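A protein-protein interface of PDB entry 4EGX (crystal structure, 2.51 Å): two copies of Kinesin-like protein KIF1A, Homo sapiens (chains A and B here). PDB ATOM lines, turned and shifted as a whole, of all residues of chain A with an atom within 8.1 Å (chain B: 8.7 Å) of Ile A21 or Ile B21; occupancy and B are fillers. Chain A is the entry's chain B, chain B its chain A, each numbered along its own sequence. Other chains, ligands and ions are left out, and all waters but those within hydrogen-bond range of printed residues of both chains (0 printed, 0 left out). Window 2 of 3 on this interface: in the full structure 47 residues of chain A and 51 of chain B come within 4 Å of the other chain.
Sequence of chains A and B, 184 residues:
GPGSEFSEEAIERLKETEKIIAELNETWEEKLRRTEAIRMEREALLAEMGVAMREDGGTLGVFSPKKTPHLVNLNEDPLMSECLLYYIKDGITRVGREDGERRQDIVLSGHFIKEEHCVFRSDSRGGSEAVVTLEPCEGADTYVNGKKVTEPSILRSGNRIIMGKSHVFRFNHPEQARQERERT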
ATOM      1  N   LEU A  14     -16.414  24.825 -10.355  1.00  0.00           N
ATOM      2  CA  LEU A  14     -15.578  26.016 -10.270  1.00  0.00           C
ATOM      3  C   LEU A  14     -16.226  27.088  -9.416  1.00  0.00           C
ATOM      4  O   LEU A  14     -15.549  27.714  -8.608  1.00  0.00           O
ATOM      5  CB  LEU A  14     -15.317  26.598 -11.656  1.00  0.00           C
ATOM      6  CG  LEU A  14     -14.841  25.716 -12.800  1.00  0.00           C
ATOM      7  CD1 LEU A  14     -15.068  26.461 -14.088  1.00  0.00           C
ATOM      8  CD2 LEU A  14     -13.392  25.303 -12.665  1.00  0.00           C
ATOM      9  N   LYS A  15     -17.528  27.319  -9.616  1.00  0.00           N
ATOM     10  CA  LYS A  15     -18.265  28.297  -8.812  1.00  0.00           C
ATOM     11  C   LYS A  15     -18.189  27.917  -7.339  1.00  0.00           C
ATOM     12  O   LYS A  15     -17.807  28.737  -6.499  1.00  0.00           O
ATOM     13  CB  LYS A  15     -19.740  28.389  -9.237  1.00  0.00           C
ATOM     14  CG  LYS A  15     -19.983  28.845 -10.657  1.00  0.00           C
ATOM     15  CD  LYS A  15     -19.893  30.345 -10.779  1.00  0.00           C
ATOM     16  CE  LYS A  15     -20.426  30.801 -12.133  1.00  0.00           C
ATOM     17  NZ  LYS A  15     -21.860  30.431 -12.321  1.00  0.00           N
ATOM     18  N   GLU A  16     -18.544  26.664  -7.040  1.00  0.00           N
ATOM     19  CA  GLU A  16     -18.389  26.117  -5.694  1.00  0.00           C
ATOM     20  C   GLU A  16     -16.996  26.396  -5.181  1.00  0.00           C
ATOM     21  O   GLU A  16     -16.836  26.847  -4.058  1.00  0.00           O
ATOM     22  CB  GLU A  16     -18.585  24.601  -5.696  1.00  0.00           C
ATOM     23  CG  GLU A  16     -20.014  24.129  -5.664  1.00  0.00           C
ATOM     24  CD  GLU A  16     -20.155  22.679  -6.120  1.00  0.00           C
ATOM     25  OE1 GLU A  16     -19.266  21.856  -5.825  1.00  0.00           O
ATOM     26  OE2 GLU A  16     -21.160  22.370  -6.780  1.00  0.00           O
ATOM     27  N   THR A  17     -16.003  26.105  -6.022  1.00  0.00           N
ATOM     28  CA  THR A  17     -14.586  26.205  -5.686  1.00  0.00           C
ATOM     29  C   THR A  17     -14.150  27.648  -5.438  1.00  0.00           C
ATOM     30  O   THR A  17     -13.246  27.894  -4.631  1.00  0.00           O
ATOM     31  CB  THR A  17     -13.706  25.566  -6.787  1.00  0.00           C
ATOM     32  OG1 THR A  17     -14.086  24.199  -6.948  1.00  0.00           O
ATOM     33  CG2 THR A  17     -12.240  25.606  -6.406  1.00  0.00           C
ATOM     34  N   GLU A  18     -14.788  28.595  -6.120  1.00  0.00           N
ATOM     35  CA  GLU A  18     -14.506  30.005  -5.874  1.00  0.00           C
ATOM     36  C   GLU A  18     -14.977  30.419  -4.476  1.00  0.00           C
ATOM     37  O   GLU A  18     -14.278  31.157  -3.762  1.00  0.00           O
ATOM     38  CB  GLU A  18     -15.145  30.866  -6.956  1.00  0.00           C
ATOM     39  CG  GLU A  18     -14.358  30.876  -8.250  1.00  0.00           C
ATOM     40  CD  GLU A  18     -15.236  31.047  -9.473  1.00  0.00           C
ATOM     41  OE1 GLU A  18     -16.278  31.747  -9.400  1.00  0.00           O
ATOM     42  OE2 GLU A  18     -14.877  30.466 -10.517  1.00  0.00           O
ATOM     43  N   LYS A  19     -16.163  29.929  -4.106  1.00  0.00           N
ATOM     44  CA  LYS A  19     -16.721  30.095  -2.762  1.00  0.00           C
ATOM     45  C   LYS A  19     -15.854  29.457  -1.684  1.00  0.00           C
ATOM     46  O   LYS A  19     -15.538  30.085  -0.668  1.00  0.00           O
ATOM     47  CB  LYS A  19     -18.122  29.492  -2.688  1.00  0.00           C
ATOM     48  CG  LYS A  19     -19.231  30.505  -2.753  1.00  0.00           C
ATOM     49  CD  LYS A  19     -20.488  29.990  -2.061  1.00  0.00           C
ATOM     50  CE  LYS A  19     -20.203  29.528  -0.629  1.00  0.00           C
ATOM     51  NZ  LYS A  19     -19.622  30.616   0.218  1.00  0.00           N
ATOM     52  N   ILE A  20     -15.467  28.209  -1.923  1.00  0.00           N
ATOM     53  CA  ILE A  20     -14.626  27.484  -0.981  1.00  0.00           C
ATOM     54  C   ILE A  20     -13.332  28.230  -0.629  1.00  0.00           C
ATOM     55  O   ILE A  20     -12.942  28.280   0.526  1.00  0.00           O
ATOM     56  CB  ILE A  20     -14.309  26.063  -1.482  1.00  0.00           C
ATOM     57  CG1 ILE A  20     -15.586  25.231  -1.534  1.00  0.00           C
ATOM     58  CG2 ILE A  20     -13.306  25.377  -0.574  1.00  0.00           C
ATOM     59  CD1 ILE A  20     -15.421  23.961  -2.208  1.00  0.00           C
ATOM     60  N   ILE A  21     -12.684  28.819  -1.619  1.00  0.00           N
ATOM     61  CA  ILE A  21     -11.389  29.430  -1.396  1.00  0.00           C
ATOM     62  C   ILE A  21     -11.508  30.667  -0.494  1.00  0.00           C
ATOM     63  O   ILE A  21     -10.659  30.889   0.373  1.00  0.00           O
ATOM     64  CB  ILE A  21     -10.666  29.726  -2.746  1.00  0.00           C
ATOM     65  CG1 ILE A  21     -10.432  28.415  -3.499  1.00  0.00           C
ATOM     66  CG2 ILE A  21      -9.337  30.444  -2.519  1.00  0.00           C
ATOM     67  CD1 ILE A  21     -10.115  28.583  -4.950  1.00  0.00           C
ATOM     68  N   ALA A  22     -12.576  31.446  -0.698  1.00  0.00           N
ATOM     69  CA  ALA A  22     -12.882  32.635   0.118  1.00  0.00           C
ATOM     70  C   ALA A  22     -13.249  32.253   1.545  1.00  0.00           C
ATOM     71  O   ALA A  22     -13.078  33.049   2.467  1.00  0.00           O
ATOM     72  CB  ALA A  22     -14.001  33.457  -0.518  1.00  0.00           C
ATOM     73  N   GLU A  23     -13.752  31.031   1.708  1.00  0.00           N
ATOM     74  CA  GLU A  23     -14.088  30.475   3.013  1.00  0.00           C
ATOM     75  C   GLU A  23     -12.868  29.879   3.671  1.00  0.00           C
ATOM     76  O   GLU A  23     -12.729  29.922   4.897  1.00  0.00           O
ATOM     77  CB  GLU A  23     -15.157  29.400   2.871  1.00  0.00           C
ATOM     78  CG  GLU A  23     -16.565  29.896   3.113  1.00  0.00           C
ATOM     79  CD  GLU A  23     -17.612  28.974   2.523  1.00  0.00           C
ATOM     80  OE1 GLU A  23     -17.335  28.334   1.490  1.00  0.00           O
ATOM     81  OE2 GLU A  23     -18.725  28.893   3.086  1.00  0.00           O
ATOM     82  N   LEU A  24     -11.994  29.302   2.851  1.00  0.00           N
ATOM     83  CA  LEU A  24     -10.708  28.820   3.323  1.00  0.00           C
ATOM     84  C   LEU A  24      -9.827  30.009   3.735  1.00  0.00           C
ATOM     85  O   LEU A  24      -9.036  29.905   4.684  1.00  0.00           O
ATOM     86  CB  LEU A  24     -10.011  27.987   2.256  1.00  0.00           C
ATOM     87  CG  LEU A  24      -8.592  27.546   2.604  1.00  0.00           C
ATOM     88  CD1 LEU A  24      -8.632  26.598   3.765  1.00  0.00           C
ATOM     89  CD2 LEU A  24      -7.903  26.886   1.448  1.00  0.00           C
ATOM     90  N   ASN A  25      -9.969  31.133   3.036  1.00  0.00           N
ATOM     91  CA  ASN A  25      -9.190  32.302   3.392  1.00  0.00           C
ATOM     92  C   ASN A  25      -9.682  32.985   4.666  1.00  0.00           C
ATOM     93  O   ASN A  25      -8.889  33.537   5.435  1.00  0.00           O
ATOM     94  CB  ASN A  25      -9.084  33.301   2.248  1.00  0.00           C
ATOM     95  CG  ASN A  25      -7.989  34.312   2.491  1.00  0.00           C
ATOM     96  OD1 ASN A  25      -6.851  33.945   2.790  1.00  0.00           O
ATOM     97  ND2 ASN A  25      -8.328  35.594   2.392  1.00  0.00           N
ATOM     98  N   GLU A  26     -10.984  32.935   4.894  1.00  0.00           N
ATOM     99  CA  GLU A  26     -11.513  33.416   6.152  1.00  0.00           C
ATOM    100  C   GLU A  26     -11.045  32.571   7.345  1.00  0.00           C
ATOM    101  O   GLU A  26     -10.598  33.129   8.357  1.00  0.00           O
ATOM    102  CB  GLU A  26     -13.033  33.549   6.098  1.00  0.00           C
ATOM    103  CG  GLU A  26     -13.478  34.943   5.697  1.00  0.00           C
ATOM    104  CD  GLU A  26     -14.936  35.014   5.323  1.00  0.00           C
ATOM    105  OE1 GLU A  26     -15.544  33.956   5.049  1.00  0.00           O
ATOM    106  OE2 GLU A  26     -15.470  36.141   5.292  1.00  0.00           O
ATOM    107  N   THR A  27     -11.106  31.242   7.214  1.00  0.00           N
ATOM    108  CA  THR A  27     -10.695  30.361   8.318  1.00  0.00           C
ATOM    109  C   THR A  27      -9.319  30.734   8.852  1.00  0.00           C
ATOM    110  O   THR A  27      -9.093  30.719  10.058  1.00  0.00           O
ATOM    111  CB  THR A  27     -10.704  28.842   7.962  1.00  0.00           C
ATOM    112  OG1 THR A  27      -9.841  28.595   6.842  1.00  0.00           O
ATOM    113  CG2 THR A  27     -12.120  28.353   7.663  1.00  0.00           C
ATOM    114  N   TRP A  28      -8.401  31.083   7.963  1.00  0.00           N
ATOM    115  CA  TRP A  28      -7.087  31.520   8.402  1.00  0.00           C
ATOM    116  C   TRP A  28      -7.099  32.915   9.016  1.00  0.00           C
ATOM    117  O   TRP A  28      -6.453  33.145  10.044  1.00  0.00           O
ATOM    118  CB  TRP A  28      -6.103  31.474   7.251  1.00  0.00           C
ATOM    119  CG  TRP A  28      -5.683  30.109   6.896  1.00  0.00           C
ATOM    120  CD1 TRP A  28      -6.136  29.369   5.859  1.00  0.00           C
ATOM    121  CD2 TRP A  28      -4.716  29.306   7.577  1.00  0.00           C
ATOM    122  NE1 TRP A  28      -5.515  28.148   5.842  1.00  0.00           N
ATOM    123  CE2 TRP A  28      -4.634  28.084   6.886  1.00  0.00           C
ATOM    124  CE3 TRP A  28      -3.912  29.503   8.702  1.00  0.00           C
ATOM    125  CZ2 TRP A  28      -3.776  27.061   7.277  1.00  0.00           C
ATOM    126  CZ3 TRP A  28      -3.062  28.485   9.093  1.00  0.00           C
ATOM    127  CH2 TRP A  28      -3.001  27.279   8.386  1.00  0.00           C
ATOM    128  N   LEU B  14      -6.371  25.124 -13.949  1.00  0.00           N
ATOM    129  CA  LEU B  14      -6.847  24.401 -12.769  1.00  0.00           C
ATOM    130  C   LEU B  14      -5.678  23.810 -11.993  1.00  0.00           C
ATOM    131  O   LEU B  14      -5.665  23.860 -10.770  1.00  0.00           O
ATOM    132  CB  LEU B  14      -7.849  23.304 -13.159  1.00  0.00           C
ATOM    133  CG  LEU B  14      -9.129  23.700 -13.923  1.00  0.00           C
ATOM    134  CD1 LEU B  14     -10.045  22.525 -14.101  1.00  0.00           C
ATOM    135  CD2 LEU B  14      -9.879  24.770 -13.189  1.00  0.00           C
ATOM    136  N   LYS B  15      -4.697  23.262 -12.700  1.00  0.00           N
ATOM    137  CA  LYS B  15      -3.498  22.738 -12.054  1.00  0.00           C
ATOM    138  C   LYS B  15      -2.724  23.860 -11.364  1.00  0.00           C
ATOM    139  O   LYS B  15      -2.153  23.654 -10.294  1.00  0.00           O
ATOM    140  CB  LYS B  15      -2.594  21.996 -13.056  1.00  0.00           C
ATOM    141  CG  LYS B  15      -3.127  20.637 -13.512  1.00  0.00           C
ATOM    142  CD  LYS B  15      -2.428  20.179 -14.776  1.00  0.00           C
ATOM    143  CE  LYS B  15      -2.584  18.675 -14.980  1.00  0.00           C
ATOM    144  NZ  LYS B  15      -1.635  17.898 -14.106  1.00  0.00           N
ATOM    145  N   GLU B  16      -2.714  25.040 -11.981  1.00  0.00           N
ATOM    146  CA  GLU B  16      -2.091  26.220 -11.383  1.00  0.00           C
ATOM    147  C   GLU B  16      -2.881  26.736 -10.176  1.00  0.00           C
ATOM    148  O   GLU B  16      -2.318  27.374  -9.303  1.00  0.00           O
ATOM    149  CB  GLU B  16      -1.931  27.338 -12.417  1.00  0.00           C
ATOM    150  CG  GLU B  16      -0.944  27.018 -13.562  1.00  0.00           C
ATOM    151  CD  GLU B  16      -1.020  28.013 -14.736  1.00  0.00           C
ATOM    152  OE1 GLU B  16      -1.839  28.965 -14.716  1.00  0.00           O
ATOM    153  OE2 GLU B  16      -0.244  27.838 -15.696  1.00  0.00           O
ATOM    154  N   THR B  17      -4.179  26.459 -10.127  1.00  0.00           N
ATOM    155  CA  THR B  17      -5.011  26.869  -8.999  1.00  0.00           C
ATOM    156  C   THR B  17      -4.797  25.919  -7.798  1.00  0.00           C
ATOM    157  O   THR B  17      -4.733  26.347  -6.642  1.00  0.00           O
ATOM    158  CB  THR B  17      -6.516  26.923  -9.422  1.00  0.00           C
ATOM    159  OG1 THR B  17      -6.651  27.667 -10.652  1.00  0.00           O
ATOM    160  CG2 THR B  17      -7.366  27.580  -8.338  1.00  0.00           C
ATOM    161  N   GLU B  18      -4.704  24.625  -8.102  1.00  0.00           N
ATOM    162  CA  GLU B  18      -4.277  23.594  -7.165  1.00  0.00           C
ATOM    163  C   GLU B  18      -2.962  23.976  -6.478  1.00  0.00           C
ATOM    164  O   GLU B  18      -2.836  23.839  -5.265  1.00  0.00           O
ATOM    165  CB  GLU B  18      -4.076  22.297  -7.932  1.00  0.00           C
ATOM    166  CG  GLU B  18      -4.536  21.056  -7.206  1.00  0.00           C
ATOM    167  CD  GLU B  18      -4.986  19.988  -8.174  1.00  0.00           C
ATOM    168  OE1 GLU B  18      -5.690  20.330  -9.137  1.00  0.00           O
ATOM    169  OE2 GLU B  18      -4.637  18.809  -7.977  1.00  0.00           O
ATOM    170  N   LYS B  19      -1.988  24.445  -7.256  1.00  0.00           N
ATOM    171  CA  LYS B  19      -0.717  24.929  -6.714  1.00  0.00           C
ATOM    172  C   LYS B  19      -0.920  26.163  -5.854  1.00  0.00           C
ATOM    173  O   LYS B  19      -0.423  26.219  -4.738  1.00  0.00           O
ATOM    174  CB  LYS B  19       0.281  25.249  -7.825  1.00  0.00           C
ATOM    175  CG  LYS B  19       1.639  25.743  -7.318  1.00  0.00           C
ATOM    176  CD  LYS B  19       2.383  24.672  -6.506  1.00  0.00           C
ATOM    177  CE  LYS B  19       2.854  23.504  -7.389  1.00  0.00           C
ATOM    178  NZ  LYS B  19       3.691  22.526  -6.647  1.00  0.00           N
ATOM    179  N   ILE B  20      -1.667  27.132  -6.382  1.00  0.00           N
ATOM    180  CA  ILE B  20      -1.988  28.374  -5.673  1.00  0.00           C
ATOM    181  C   ILE B  20      -2.697  28.148  -4.324  1.00  0.00           C
ATOM    182  O   ILE B  20      -2.466  28.898  -3.362  1.00  0.00           O
ATOM    183  CB  ILE B  20      -2.798  29.335  -6.562  1.00  0.00           C
ATOM    184  CG1 ILE B  20      -1.956  29.786  -7.758  1.00  0.00           C
ATOM    185  CG2 ILE B  20      -3.220  30.553  -5.779  1.00  0.00           C
ATOM    186  CD1 ILE B  20      -2.740  30.490  -8.883  1.00  0.00           C
ATOM    187  N   ILE B  21      -3.536  27.116  -4.259  1.00  0.00           N
ATOM    188  CA  ILE B  21      -4.173  26.702  -3.007  1.00  0.00           C
ATOM    189  C   ILE B  21      -3.164  26.041  -2.059  1.00  0.00           C
ATOM    190  O   ILE B  21      -3.155  26.326  -0.864  1.00  0.00           O
ATOM    191  CB  ILE B  21      -5.409  25.807  -3.247  1.00  0.00           C
ATOM    192  CG1 ILE B  21      -6.513  26.614  -3.939  1.00  0.00           C
ATOM    193  CG2 ILE B  21      -5.937  25.249  -1.921  1.00  0.00           C
ATOM    194  CD1 ILE B  21      -7.699  25.812  -4.403  1.00  0.00           C
ATOM    195  N   ALA B  22      -2.308  25.172  -2.588  1.00  0.00           N
ATOM    196  CA  ALA B  22      -1.244  24.593  -1.787  1.00  0.00           C
ATOM    197  C   ALA B  22      -0.341  25.707  -1.267  1.00  0.00           C
ATOM    198  O   ALA B  22       0.014  25.724  -0.082  1.00  0.00           O
ATOM    199  CB  ALA B  22      -0.463  23.605  -2.584  1.00  0.00           C
ATOM    200  N   GLU B  23      -0.001  26.654  -2.144  1.00  0.00           N
ATOM    201  CA  GLU B  23       0.744  27.845  -1.744  1.00  0.00           C
ATOM    202  C   GLU B  23      -0.001  28.672  -0.717  1.00  0.00           C
ATOM    203  O   GLU B  23       0.614  29.221   0.200  1.00  0.00           O
ATOM    204  CB  GLU B  23       1.036  28.721  -2.941  1.00  0.00           C
ATOM    205  CG  GLU B  23       2.472  28.739  -3.345  1.00  0.00           C
ATOM    206  CD  GLU B  23       2.630  29.123  -4.785  1.00  0.00           C
ATOM    207  OE1 GLU B  23       1.590  29.355  -5.456  1.00  0.00           O
ATOM    208  OE2 GLU B  23       3.798  29.178  -5.252  1.00  0.00           O
ATOM    209  N   LEU B  24      -1.320  28.770  -0.887  1.00  0.00           N
ATOM    210  CA  LEU B  24      -2.153  29.528   0.039  1.00  0.00           C
ATOM    211  C   LEU B  24      -2.107  28.904   1.434  1.00  0.00           C
ATOM    212  O   LEU B  24      -1.757  29.577   2.407  1.00  0.00           O
ATOM    213  CB  LEU B  24      -3.588  29.619  -0.475  1.00  0.00           C
ATOM    214  CG  LEU B  24      -4.579  30.421   0.356  1.00  0.00           C
ATOM    215  CD1 LEU B  24      -5.520  31.119  -0.577  1.00  0.00           C
ATOM    216  CD2 LEU B  24      -5.353  29.517   1.309  1.00  0.00           C
ATOM    217  N   ASN B  25      -2.459  27.622   1.515  1.00  0.00           N
ATOM    218  CA  ASN B  25      -2.304  26.863   2.738  1.00  0.00           C
ATOM    219  C   ASN B  25      -0.928  27.140   3.334  1.00  0.00           C
ATOM    220  O   ASN B  25      -0.808  27.459   4.520  1.00  0.00           O
ATOM    221  CB  ASN B  25      -2.448  25.366   2.462  1.00  0.00           C
ATOM    222  CG  ASN B  25      -3.880  24.945   2.180  1.00  0.00           C
ATOM    223  OD1 ASN B  25      -4.839  25.491   2.733  1.00  0.00           O
ATOM    224  ND2 ASN B  25      -4.027  23.945   1.320  1.00  0.00           N
ATOM    225  N   GLU B  26       0.095  27.040   2.483  1.00  0.00           N
ATOM    226  CA  GLU B  26       1.492  27.134   2.891  1.00  0.00           C
ATOM    227  C   GLU B  26       1.903  28.449   3.551  1.00  0.00           C
ATOM    228  O   GLU B  26       2.513  28.426   4.629  1.00  0.00           O
ATOM    229  CB  GLU B  26       2.414  26.814   1.715  1.00  0.00           C
ATOM    230  CG  GLU B  26       3.112  25.477   1.844  1.00  0.00           C
ATOM    231  CD  GLU B  26       3.294  24.765   0.519  1.00  0.00           C
ATOM    232  OE1 GLU B  26       3.520  25.439  -0.515  1.00  0.00           O
ATOM    233  OE2 GLU B  26       3.208  23.516   0.515  1.00  0.00           O
ATOM    234  N   THR B  27       1.580  29.585   2.929  1.00  0.00           N
ATOM    235  CA  THR B  27       2.038  30.878   3.470  1.00  0.00           C
ATOM    236  C   THR B  27       1.235  31.308   4.686  1.00  0.00           C
ATOM    237  O   THR B  27       1.743  32.020   5.562  1.00  0.00           O
ATOM    238  CB  THR B  27       2.069  32.039   2.425  1.00  0.00           C
ATOM    239  OG1 THR B  27       0.755  32.620   2.286  1.00  0.00           O
ATOM    240  CG2 THR B  27       2.598  31.568   1.073  1.00  0.00           C
ATOM    241  N   TRP B  28      -0.019  30.877   4.735  1.00  0.00           N
ATOM    242  CA  TRP B  28      -0.852  31.154   5.888  1.00  0.00           C
ATOM    243  C   TRP B  28      -0.341  30.424   7.127  1.00  0.00           C
ATOM    244  O   TRP B  28      -0.267  31.012   8.209  1.00  0.00           O
ATOM    245  CB  TRP B  28      -2.295  30.761   5.621  1.00  0.00           C
ATOM    246  CG  TRP B  28      -3.185  31.881   5.222  1.00  0.00           C
ATOM    247  CD1 TRP B  28      -3.946  31.952   4.094  1.00  0.00           C
ATOM    248  CD2 TRP B  28      -3.437  33.087   5.958  1.00  0.00           C
ATOM    249  NE1 TRP B  28      -4.655  33.128   4.077  1.00  0.00           N
ATOM    250  CE2 TRP B  28      -4.360  33.845   5.207  1.00  0.00           C
ATOM    251  CE3 TRP B  28      -2.971  33.600   7.177  1.00  0.00           C
ATOM    252  CZ2 TRP B  28      -4.820  35.094   5.625  1.00  0.00           C
ATOM    253  CZ3 TRP B  28      -3.429  34.845   7.594  1.00  0.00           C
ATOM    254  CH2 TRP B  28      -4.345  35.578   6.817  1.00  0.00           C
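Ile A21 touches just one residue of chain B: Ile B21 (3.7 Å). No residue of chain B comes within 4 Å of Ala A22. Printed residues of chain B within 4 Å of Leu A24: Leu B24 (3.7 Å) and Asn B25 (3.6 Å). Printed residues of chain A within 4 Å of Leu B14: Leu A14 (3.6 Å). Of chain A, only Ile A21 comes within 4 Å of Ile B21. Of the printed residues of chain A, Trp B28 touches Asn A25 (2.7 Å) and Trp A28 (3.4 Å). The nearest residue of chain B that does not touch Ile A21 is Leu B24 (4.3 Å).
The side-chain amide nitrogen (ND2) of Asn B25 is in hydrogen-bond range of the backbone carbonyl oxygen (O) of Ile B21 (3.3 Å). O of Leu A24 lies within hydrogen-bond range of OG1 of Thr A27 (2.6 Å).
Of the 15 printed residues of chain A, 5 touch a printed residue of chain B. Hydrophobic or aromatic side chains of chain A within 4 Å of the printed part of chain B: Leu A14, Ile A21, Leu A24 and Trp A28. Of the 15 printed residues of chain B, 5 touch a printed residue of chain A. Hydrophobic or aromatic side chains of chain B that line the printed part of chain A: Leu B14, Ile B21, Leu B24 and Trp B28. Among the printed residues, no Asp or Glu carboxylate lies within 4 Å of a Lys or Arg side-chain nitrogen of the other chain.
Ile B21 touches its own counterpart, Ile A21. Leu B24 touches its own counterpart, Leu A24. Leu A24 touches Asn B25, but with the chains exchanged Asn A25 does not touch Leu B24 (4.6 Å). Asn A25 touches Trp B28, but with the chains exchanged Trp A28 does not touch Asn B25 (4.1 Å). Positions printed for both chains: 14, 15, 16, 17, 18, 19, 20, 21, 22, 23, 24, 25, 26, 27 and 28.
Among the printed residues, pairs that only touch across the chains: Trp A28 with Trp B28, Leu A14 with Leu B14, Leu A24 with Asn B25, Leu A24 with Leu B24 and Ile A21 with Ile B21.
The indole nitrogen (NE1) of Trp B28 sits at hydrogen-bond distance from the side-chain amide oxygen (OD1) of Asn A25, 2.7 Å away.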
